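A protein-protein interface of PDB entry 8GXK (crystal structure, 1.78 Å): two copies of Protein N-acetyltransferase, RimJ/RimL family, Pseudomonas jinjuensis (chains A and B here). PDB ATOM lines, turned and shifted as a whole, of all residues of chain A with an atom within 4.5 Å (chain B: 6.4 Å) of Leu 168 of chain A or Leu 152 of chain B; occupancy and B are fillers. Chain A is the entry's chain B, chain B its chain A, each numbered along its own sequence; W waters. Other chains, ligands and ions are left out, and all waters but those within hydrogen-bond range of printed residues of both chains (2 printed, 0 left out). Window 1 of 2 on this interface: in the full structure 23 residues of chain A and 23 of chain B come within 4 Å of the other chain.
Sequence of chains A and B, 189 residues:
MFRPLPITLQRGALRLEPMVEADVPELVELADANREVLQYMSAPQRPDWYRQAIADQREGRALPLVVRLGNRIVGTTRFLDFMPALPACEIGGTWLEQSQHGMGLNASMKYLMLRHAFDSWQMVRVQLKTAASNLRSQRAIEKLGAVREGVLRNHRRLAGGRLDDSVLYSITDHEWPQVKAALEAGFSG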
ATOM      1  N   ARG A 125     -13.477  20.325  -5.164  1.00  0.00           N
ATOM      2  CA  ARG A 125     -13.477  18.884  -4.964  1.00  0.00           C
ATOM      3  C   ARG A 125     -12.658  18.579  -3.724  1.00  0.00           C
ATOM      4  O   ARG A 125     -11.537  19.080  -3.610  1.00  0.00           O
ATOM      5  CB  ARG A 125     -12.841  18.182  -6.143  1.00  0.00           C
ATOM      6  CG  ARG A 125     -12.671  16.667  -5.967  1.00  0.00           C
ATOM      7  CD  ARG A 125     -11.751  16.054  -7.083  1.00  0.00           C
ATOM      8  NE  ARG A 125     -11.407  14.672  -6.783  1.00  0.00           N
ATOM      9  CZ  ARG A 125     -12.215  13.644  -7.020  1.00  0.00           C
ATOM     10  NH1 ARG A 125     -11.838  12.434  -6.669  1.00  0.00           N
ATOM     11  NH2 ARG A 125     -13.423  13.821  -7.545  1.00  0.00           N
ATOM     12  N   GLN A 127     -11.582  14.877  -1.894  1.00  0.00           N
ATOM     13  CA  GLN A 127     -11.748  13.436  -2.041  1.00  0.00           C
ATOM     14  C   GLN A 127     -11.348  12.717  -0.756  1.00  0.00           C
ATOM     15  O   GLN A 127     -10.619  13.249   0.082  1.00  0.00           O
ATOM     16  CB  GLN A 127     -10.973  12.887  -3.254  1.00  0.00           C
ATOM     17  CG  GLN A 127      -9.481  12.796  -3.126  1.00  0.00           C
ATOM     18  CD  GLN A 127      -8.777  12.280  -4.349  1.00  0.00           C
ATOM     19  OE1 GLN A 127      -9.271  12.389  -5.466  1.00  0.00           O
ATOM     20  NE2 GLN A 127      -7.564  11.757  -4.130  1.00  0.00           N
ATOM     21  N   LEU A 128     -11.876  11.504  -0.578  1.00  0.00           N
ATOM     22  CA  LEU A 128     -11.521  10.681   0.564  1.00  0.00           C
ATOM     23  C   LEU A 128     -11.445   9.265   0.062  1.00  0.00           C
ATOM     24  O   LEU A 128     -12.231   8.896  -0.811  1.00  0.00           O
ATOM     25  CB  LEU A 128     -12.560  10.763   1.673  1.00  0.00           C
ATOM     26  CG  LEU A 128     -12.929  12.165   2.162  1.00  0.00           C
ATOM     27  CD1 LEU A 128     -14.117  12.688   1.312  1.00  0.00           C
ATOM     28  CD2 LEU A 128     -13.250  12.092   3.603  1.00  0.00           C
ATOM     29  N   LYS A 129     -10.497   8.475   0.564  1.00  0.00           N
ATOM     30  CA  LYS A 129     -10.423   7.097   0.120  1.00  0.00           C
ATOM     31  C   LYS A 129     -10.007   6.204   1.277  1.00  0.00           C
ATOM     32  O   LYS A 129      -9.420   6.653   2.270  1.00  0.00           O
ATOM     33  CB  LYS A 129      -9.459   6.938  -1.058  1.00  0.00           C
ATOM     34  CG  LYS A 129      -8.038   7.164  -0.754  1.00  0.00           C
ATOM     35  CD  LYS A 129      -7.229   7.247  -2.049  1.00  0.00           C
ATOM     36  CE  LYS A 129      -5.767   7.258  -1.753  1.00  0.00           C
ATOM     37  NZ  LYS A 129      -5.171   8.577  -2.063  1.00  0.00           N
ATOM     38  N   VAL A 147     -19.794  10.999  -2.231  1.00  0.00           N
ATOM     39  CA  VAL A 147     -20.281  10.158  -3.315  1.00  0.00           C
ATOM     40  C   VAL A 147     -19.205   9.148  -3.668  1.00  0.00           C
ATOM     41  O   VAL A 147     -18.036   9.508  -3.819  1.00  0.00           O
ATOM     42  CB  VAL A 147     -20.658  11.008  -4.541  1.00  0.00           C
ATOM     43  CG1 VAL A 147     -20.977  10.121  -5.739  1.00  0.00           C
ATOM     44  CG2 VAL A 147     -21.789  11.953  -4.214  1.00  0.00           C
ATOM     45  N   ARG A 148     -19.596   7.891  -3.794  1.00  0.00           N
ATOM     46  CA  ARG A 148     -18.671   6.809  -4.114  1.00  0.00           C
ATOM     47  C   ARG A 148     -18.360   6.830  -5.616  1.00  0.00           C
ATOM     48  O   ARG A 148     -19.214   6.502  -6.441  1.00  0.00           O
ATOM     49  CB  ARG A 148     -19.278   5.472  -3.722  1.00  0.00           C
ATOM     50  CG  ARG A 148     -18.321   4.313  -3.999  1.00  0.00           C
ATOM     51  CD  ARG A 148     -19.047   3.044  -4.218  1.00  0.00           C
ATOM     52  NE  ARG A 148     -18.958   2.176  -3.068  1.00  0.00           N
ATOM     53  CZ  ARG A 148     -18.391   0.984  -3.073  1.00  0.00           C
ATOM     54  NH1 ARG A 148     -18.367   0.273  -1.963  1.00  0.00           N
ATOM     55  NH2 ARG A 148     -17.822   0.513  -4.164  1.00  0.00           N
ATOM     56  N   GLU A 149     -17.130   7.175  -5.984  1.00  0.00           N
ATOM     57  CA  GLU A 149     -16.781   7.275  -7.394  1.00  0.00           C
ATOM     58  C   GLU A 149     -16.337   5.941  -8.001  1.00  0.00           C
ATOM     59  O   GLU A 149     -16.609   5.675  -9.182  1.00  0.00           O
ATOM     60  CB  GLU A 149     -15.705   8.358  -7.554  1.00  0.00           C
ATOM     61  CG  GLU A 149     -16.236   9.739  -7.204  1.00  0.00           C
ATOM     62  CD  GLU A 149     -15.233  10.852  -7.329  1.00  0.00           C
ATOM     63  OE1 GLU A 149     -14.020  10.649  -7.146  1.00  0.00           O
ATOM     64  OE2 GLU A 149     -15.672  11.993  -7.549  1.00  0.00           O
ATOM     65  N   GLY A 150     -15.671   5.090  -7.240  1.00  0.00           N
ATOM     66  CA  GLY A 150     -15.408   3.749  -7.727  1.00  0.00           C
ATOM     67  C   GLY A 150     -14.332   3.074  -6.910  1.00  0.00           C
ATOM     68  O   GLY A 150     -13.941   3.554  -5.852  1.00  0.00           O
ATOM     69  N   LEU A 152     -10.560   1.417  -6.883  1.00  0.00           N
ATOM     70  CA  LEU A 152      -9.254   1.455  -7.520  1.00  0.00           C
ATOM     71  C   LEU A 152      -8.496   0.182  -7.155  1.00  0.00           C
ATOM     72  O   LEU A 152      -8.221  -0.076  -5.981  1.00  0.00           O
ATOM     73  CB  LEU A 152      -8.455   2.684  -7.105  1.00  0.00           C
ATOM     74  CG  LEU A 152      -9.209   4.006  -7.041  1.00  0.00           C
ATOM     75  CD1 LEU A 152      -8.112   5.146  -7.038  1.00  0.00           C
ATOM     76  CD2 LEU A 152     -10.293   4.308  -7.924  1.00  0.00           C
ATOM     77  N   SER A 166      -8.746   0.291  -3.195  1.00  0.00           N
ATOM     78  CA  SER A 166      -9.247   1.485  -2.503  1.00  0.00           C
ATOM     79  C   SER A 166     -10.651   1.776  -2.992  1.00  0.00           C
ATOM     80  O   SER A 166     -10.950   1.570  -4.169  1.00  0.00           O
ATOM     81  CB  SER A 166      -8.399   2.762  -2.706  1.00  0.00           C
ATOM     82  OG  SER A 166      -7.134   2.626  -2.095  1.00  0.00           O
ATOM     83  N   VAL A 167     -11.528   2.210  -2.087  1.00  0.00           N
ATOM     84  CA  VAL A 167     -12.780   2.856  -2.468  1.00  0.00           C
ATOM     85  C   VAL A 167     -12.587   4.360  -2.417  1.00  0.00           C
ATOM     86  O   VAL A 167     -12.236   4.914  -1.373  1.00  0.00           O
ATOM     87  CB  VAL A 167     -13.926   2.440  -1.553  1.00  0.00           C
ATOM     88  CG1 VAL A 167     -15.181   2.975  -2.043  1.00  0.00           C
ATOM     89  CG2 VAL A 167     -13.904   0.936  -1.421  1.00  0.00           C
ATOM     90  N   LEU A 168     -12.907   5.021  -3.530  1.00  0.00           N
ATOM     91  CA  LEU A 168     -12.661   6.438  -3.718  1.00  0.00           C
ATOM     92  C   LEU A 168     -13.993   7.174  -3.680  1.00  0.00           C
ATOM     93  O   LEU A 168     -14.936   6.800  -4.391  1.00  0.00           O
ATOM     94  CB  LEU A 168     -11.938   6.723  -5.040  1.00  0.00           C
ATOM     95  CG  LEU A 168     -11.750   8.226  -5.320  1.00  0.00           C
ATOM     96  CD1 LEU A 168     -10.939   8.898  -4.331  1.00  0.00           C
ATOM     97  CD2 LEU A 168     -11.074   8.370  -6.713  1.00  0.00           C
ATOM     98  N   TYR A 169     -14.059   8.197  -2.830  1.00  0.00           N
ATOM     99  CA  TYR A 169     -15.235   9.058  -2.713  1.00  0.00           C
ATOM    100  C   TYR A 169     -14.875  10.514  -2.942  1.00  0.00           C
ATOM    101  O   TYR A 169     -13.730  10.908  -2.756  1.00  0.00           O
ATOM    102  CB  TYR A 169     -15.858   9.004  -1.312  1.00  0.00           C
ATOM    103  CG  TYR A 169     -16.172   7.620  -0.789  1.00  0.00           C
ATOM    104  CD1 TYR A 169     -17.466   7.154  -0.781  1.00  0.00           C
ATOM    105  CD2 TYR A 169     -15.190   6.803  -0.255  1.00  0.00           C
ATOM    106  CE1 TYR A 169     -17.775   5.942  -0.267  1.00  0.00           C
ATOM    107  CE2 TYR A 169     -15.508   5.551   0.216  1.00  0.00           C
ATOM    108  CZ  TYR A 169     -16.787   5.143   0.207  1.00  0.00           C
ATOM    109  OH  TYR A 169     -17.098   3.925   0.705  1.00  0.00           O
ATOM    110  N   LYS B 129      -5.920   8.602 -16.804  1.00  0.00           N
ATOM    111  CA  LYS B 129      -7.149   9.380 -16.690  1.00  0.00           C
ATOM    112  C   LYS B 129      -7.252  10.371 -17.844  1.00  0.00           C
ATOM    113  O   LYS B 129      -6.252  10.762 -18.440  1.00  0.00           O
ATOM    114  CB  LYS B 129      -7.196  10.085 -15.337  1.00  0.00           C
ATOM    115  CG  LYS B 129      -6.203  11.164 -15.226  1.00  0.00           C
ATOM    116  CD  LYS B 129      -6.100  11.695 -13.802  1.00  0.00           C
ATOM    117  CE  LYS B 129      -5.471  10.637 -12.915  1.00  0.00           C
ATOM    118  NZ  LYS B 129      -4.541  11.200 -11.906  1.00  0.00           N
ATOM    119  N   GLY B 150     -13.956   4.723 -12.563  1.00  0.00           N
ATOM    120  CA  GLY B 150     -15.026   5.601 -12.151  1.00  0.00           C
ATOM    121  C   GLY B 150     -14.818   6.985 -12.700  1.00  0.00           C
ATOM    122  O   GLY B 150     -13.860   7.264 -13.420  1.00  0.00           O
ATOM    123  N   VAL B 151     -15.782   7.831 -12.386  1.00  0.00           N
ATOM    124  CA  VAL B 151     -15.791   9.208 -12.841  1.00  0.00           C
ATOM    125  C   VAL B 151     -15.431  10.059 -11.643  1.00  0.00           C
ATOM    126  O   VAL B 151     -16.066   9.940 -10.588  1.00  0.00           O
ATOM    127  CB  VAL B 151     -17.148   9.610 -13.423  1.00  0.00           C
ATOM    128  CG1 VAL B 151     -17.168  11.099 -13.671  1.00  0.00           C
ATOM    129  CG2 VAL B 151     -17.379   8.845 -14.687  1.00  0.00           C
ATOM    130  N   LEU B 152     -14.359  10.843 -11.767  1.00  0.00           N
ATOM    131  CA  LEU B 152     -13.931  11.754 -10.704  1.00  0.00           C
ATOM    132  C   LEU B 152     -14.445  13.151 -11.027  1.00  0.00           C
ATOM    133  O   LEU B 152     -14.015  13.760 -12.014  1.00  0.00           O
ATOM    134  CB  LEU B 152     -12.414  11.797 -10.543  1.00  0.00           C
ATOM    135  CG  LEU B 152     -11.682  10.480 -10.572  1.00  0.00           C
ATOM    136  CD1 LEU B 152     -10.215  10.694 -10.238  1.00  0.00           C
ATOM    137  CD2 LEU B 152     -12.229   9.415  -9.766  1.00  0.00           C
ATOM    138  N   ARG B 153     -15.340  13.661 -10.179  1.00  0.00           N
ATOM    139  CA  ARG B 153     -16.011  14.920 -10.437  1.00  0.00           C
ATOM    140  C   ARG B 153     -15.111  16.080 -10.071  1.00  0.00           C
ATOM    141  O   ARG B 153     -14.352  16.018  -9.105  1.00  0.00           O
ATOM    142  CB  ARG B 153     -17.312  14.967  -9.658  1.00  0.00           C
ATOM    143  CG  ARG B 153     -18.351  14.012 -10.259  1.00  0.00           C
ATOM    144  CD  ARG B 153     -18.818  12.843  -9.364  1.00  0.00           C
ATOM    145  NE  ARG B 153     -18.439  12.983  -7.960  1.00  0.00           N
ATOM    146  CZ  ARG B 153     -19.244  13.502  -7.064  1.00  0.00           C
ATOM    147  NH1 ARG B 153     -20.454  13.856  -7.474  1.00  0.00           N
ATOM    148  NH2 ARG B 153     -18.856  13.637  -5.803  1.00  0.00           N
ATOM    149  N   ASN B 154     -15.190  17.129 -10.878  1.00  0.00           N
ATOM    150  CA  ASN B 154     -14.458  18.383 -10.702  1.00  0.00           C
ATOM    151  C   ASN B 154     -12.970  18.176 -10.486  1.00  0.00           C
ATOM    152  O   ASN B 154     -12.393  18.670  -9.517  1.00  0.00           O
ATOM    153  CB  ASN B 154     -15.016  19.189  -9.524  1.00  0.00           C
ATOM    154  CG  ASN B 154     -16.387  19.798  -9.817  1.00  0.00           C
ATOM    155  OD1 ASN B 154     -16.946  19.608 -10.911  1.00  0.00           O
ATOM    156  ND2 ASN B 154     -16.970  20.455  -8.809  1.00  0.00           N
ATOM    157  N   HIS B 155     -12.339  17.522 -11.453  1.00  0.00           N
ATOM    158  CA  HIS B 155     -11.040  16.911 -11.248  1.00  0.00           C
ATOM    159  C   HIS B 155     -10.018  17.452 -12.227  1.00  0.00           C
ATOM    160  O   HIS B 155      -8.845  17.068 -12.174  1.00  0.00           O
ATOM    161  CB  HIS B 155     -11.156  15.380 -11.377  1.00  0.00           C
ATOM    162  CG  HIS B 155      -9.923  14.639 -10.956  1.00  0.00           C
ATOM    163  ND1 HIS B 155      -9.038  14.077 -11.848  1.00  0.00           N
ATOM    164  CD2 HIS B 155      -9.418  14.395  -9.726  1.00  0.00           C
ATOM    165  CE1 HIS B 155      -8.053  13.502 -11.188  1.00  0.00           C
ATOM    166  NE2 HIS B 155      -8.261  13.675  -9.899  1.00  0.00           N
ATOM    167  N   ARG B 156     -10.414  18.376 -13.091  1.00  0.00           N
ATOM    168  CA  ARG B 156      -9.490  18.906 -14.083  1.00  0.00           C
ATOM    169  C   ARG B 156     -10.046  20.196 -14.667  1.00  0.00           C
ATOM    170  O   ARG B 156     -11.260  20.409 -14.706  1.00  0.00           O
ATOM    171  CB  ARG B 156      -9.249  17.891 -15.195  1.00  0.00           C
ATOM    172  CG  ARG B 156     -10.415  17.765 -16.094  1.00  0.00           C
ATOM    173  CD  ARG B 156     -10.162  16.849 -17.281  1.00  0.00           C
ATOM    174  NE  ARG B 156      -9.602  15.612 -16.774  1.00  0.00           N
ATOM    175  CZ  ARG B 156      -8.422  15.122 -17.107  1.00  0.00           C
ATOM    176  NH1 ARG B 156      -7.670  15.729 -18.014  1.00  0.00           N
ATOM    177  NH2 ARG B 156      -8.030  13.996 -16.549  1.00  0.00           N
ATOM    178  N   ASP B 164     -14.010  20.210 -15.646  1.00  0.00           N
ATOM    179  CA  ASP B 164     -14.536  18.962 -16.177  1.00  0.00           C
ATOM    180  C   ASP B 164     -14.268  17.858 -15.160  1.00  0.00           C
ATOM    181  O   ASP B 164     -13.430  18.002 -14.259  1.00  0.00           O
ATOM    182  CB  ASP B 164     -13.909  18.654 -17.547  1.00  0.00           C
ATOM    183  CG  ASP B 164     -14.703  17.620 -18.322  1.00  0.00           C
ATOM    184  OD1 ASP B 164     -15.752  17.151 -17.833  1.00  0.00           O
ATOM    185  OD2 ASP B 164     -14.293  17.200 -19.415  1.00  0.00           O
ATOM    186  N   ASP B 165     -15.034  16.785 -15.282  1.00  0.00           N
ATOM    187  CA  ASP B 165     -14.746  15.526 -14.626  1.00  0.00           C
ATOM    188  C   ASP B 165     -13.610  14.788 -15.341  1.00  0.00           C
ATOM    189  O   ASP B 165     -13.251  15.100 -16.478  1.00  0.00           O
ATOM    190  CB  ASP B 165     -16.002  14.668 -14.611  1.00  0.00           C
ATOM    191  CG  ASP B 165     -17.212  15.371 -13.953  1.00  0.00           C
ATOM    192  OD1 ASP B 165     -17.033  16.347 -13.197  1.00  0.00           O
ATOM    193  OD2 ASP B 165     -18.350  14.896 -14.156  1.00  0.00           O
ATOM    194  N   SER B 166     -13.028  13.811 -14.644  1.00  0.00           N
ATOM    195  CA  SER B 166     -12.071  12.887 -15.242  1.00  0.00           C
ATOM    196  C   SER B 166     -12.661  11.491 -15.204  1.00  0.00           C
ATOM    197  O   SER B 166     -13.328  11.107 -14.237  1.00  0.00           O
ATOM    198  CB  SER B 166     -10.717  12.847 -14.521  1.00  0.00           C
ATOM    199  OG  SER B 166     -10.016  14.065 -14.625  1.00  0.00           O
ATOM    200  N   VAL B 167     -12.328  10.696 -16.209  1.00  0.00           N
ATOM    201  CA  VAL B 167     -12.569   9.258 -16.161  1.00  0.00           C
ATOM    202  C   VAL B 167     -11.249   8.569 -15.832  1.00  0.00           C
ATOM    203  O   VAL B 167     -10.235   8.808 -16.492  1.00  0.00           O
ATOM    204  CB  VAL B 167     -13.146   8.744 -17.491  1.00  0.00           C
ATOM    205  CG1 VAL B 167     -13.457   7.274 -17.396  1.00  0.00           C
ATOM    206  CG2 VAL B 167     -14.432   9.526 -17.852  1.00  0.00           C
ATOM    207  N   LEU B 168     -11.265   7.686 -14.838  1.00  0.00           N
ATOM    208  CA  LEU B 168     -10.065   7.014 -14.342  1.00  0.00           C
ATOM    209  C   LEU B 168     -10.117   5.554 -14.761  1.00  0.00           C
ATOM    210  O   LEU B 168     -11.145   4.887 -14.579  1.00  0.00           O
ATOM    211  CB  LEU B 168      -9.958   7.108 -12.807  1.00  0.00           C
ATOM    212  CG  LEU B 168      -8.789   6.352 -12.139  1.00  0.00           C
ATOM    213  CD1 LEU B 168      -7.490   7.006 -12.422  1.00  0.00           C
ATOM    214  CD2 LEU B 168      -9.061   6.384 -10.585  1.00  0.00           C
HETATM  215  O   HOH W   1     -18.163   6.813 -10.837  1.00  0.00           O
HETATM  216  O   HOH W   2      -7.467  12.470  -7.515  1.00  0.00           O
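Among the printed residues, pairs that only touch across the chains: Glu 149 of chain A with Gly 150 of chain B (3.4 Å), Glu 149 of chain A with Val 151 of chain B (3.4 Å), Glu 149 of chain A with Leu 152 of chain B (3.4 Å), Leu 168 of chain A with Leu 152 of chain B (3.4 Å), Val 147 of chain A with Arg 153 of chain B (3.4 Å), Arg 125 of chain A with Asn 154 of chain B (3.4 Å), Arg 125 of chain A with His 155 of chain B (3.6 Å), Leu 152 of chain A with Leu 168 of chain B (3.6 Å) and Arg 125 of chain A with Leu 152 of chain B (3.7 Å).
Leu 152 of chain A touches Leu 168 of chain B, and with the chains exchanged Leu 168 of chain A touches Leu 152 of chain B.
The backbone NH (N) of Leu 168 of chain B sits at hydrogen-bond distance from the backbone carbonyl oxygen (O) of Gly 150 of chain B, at 3.0 Å.
The side-chain hydroxyl of Ser 166 of chain B lies within hydrogen-bond range of a ring nitrogen (ND1) of His 155 of chain B, at 2.9 Å.
N of Leu 152 of chain A lies within hydrogen-bond range of O of Ser 166 of chain A, at 2.7 Å.
The guanidinium group of Arg 125 of chain A is in salt-bridge range of the side-chain carboxylate of Glu 149 of chain A, at 2.9 Å.
The backbone NH (N) of His 155 of chain B is in hydrogen-bond range of the backbone carbonyl oxygen (O) of Asp 164 of chain B (3.0 Å).
N of Leu 152 of chain B is in hydrogen-bond range of O of Ser 166 of chain B, 2.7 Å away.
NE of Arg 153 of chain B lies within salt-bridge range of OE2 of Glu 149 of chain A, 3.0 Å away.
The backbone carbonyl oxygen of Arg 153 of chain B is in hydrogen-bond range of the guanidinium group of Arg 125 of chain A (2.9 Å).
Of the 13 printed residues of chain B, 7 touch a printed residue of chain A.
Hydrophobic or aromatic side chains of chain B that line the printed part of chain A: Leu 152, His 155 and Leu 168.
Of the 13 printed residues of chain A, 5 touch a printed residue of chain B.
Hydrophobic or aromatic side chains of chain A within 4 Å of the printed part of chain B: Val 147, Leu 152 and Leu 168.
Among the printed residues, 11 pairs touch across the chains.
Among the printed residues, Asp or Glu carboxylates within 4 Å of a Lys or Arg side-chain nitrogen of the other chain: Glu 149 of chain A with Arg 153 of chain B (3.0 Å).
Leu 152 of chain B touches just these residues of chain A: Arg 125, Glu 149 and Leu 168.
Of the printed residues of chain A, Asn 154 of chain B touches Arg 125 (3.4 Å).
Of the printed residues of chain B, Arg 125 of chain A touches Leu 152, Arg 153, Asn 154 and His 155.
The nearest residue of chain B that does not touch Leu 168 of chain A is Leu 168 of chain B (4.8 Å).
The nearest printed residue of chain A that does not touch Leu 152 of chain B is Gln 127 of chain A (5.2 Å).
Water W1 bridges O of Glu 149 of chain A (2.5 Å) and N of Val 151 of chain B (3.0 Å).
Water W2 lies within hydrogen-bond range of the side-chain amide oxygen (OE1) of Gln 127 of chain A (2.7 Å) and a ring nitrogen (NE2) of His 155 of chain B (2.8 Å).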
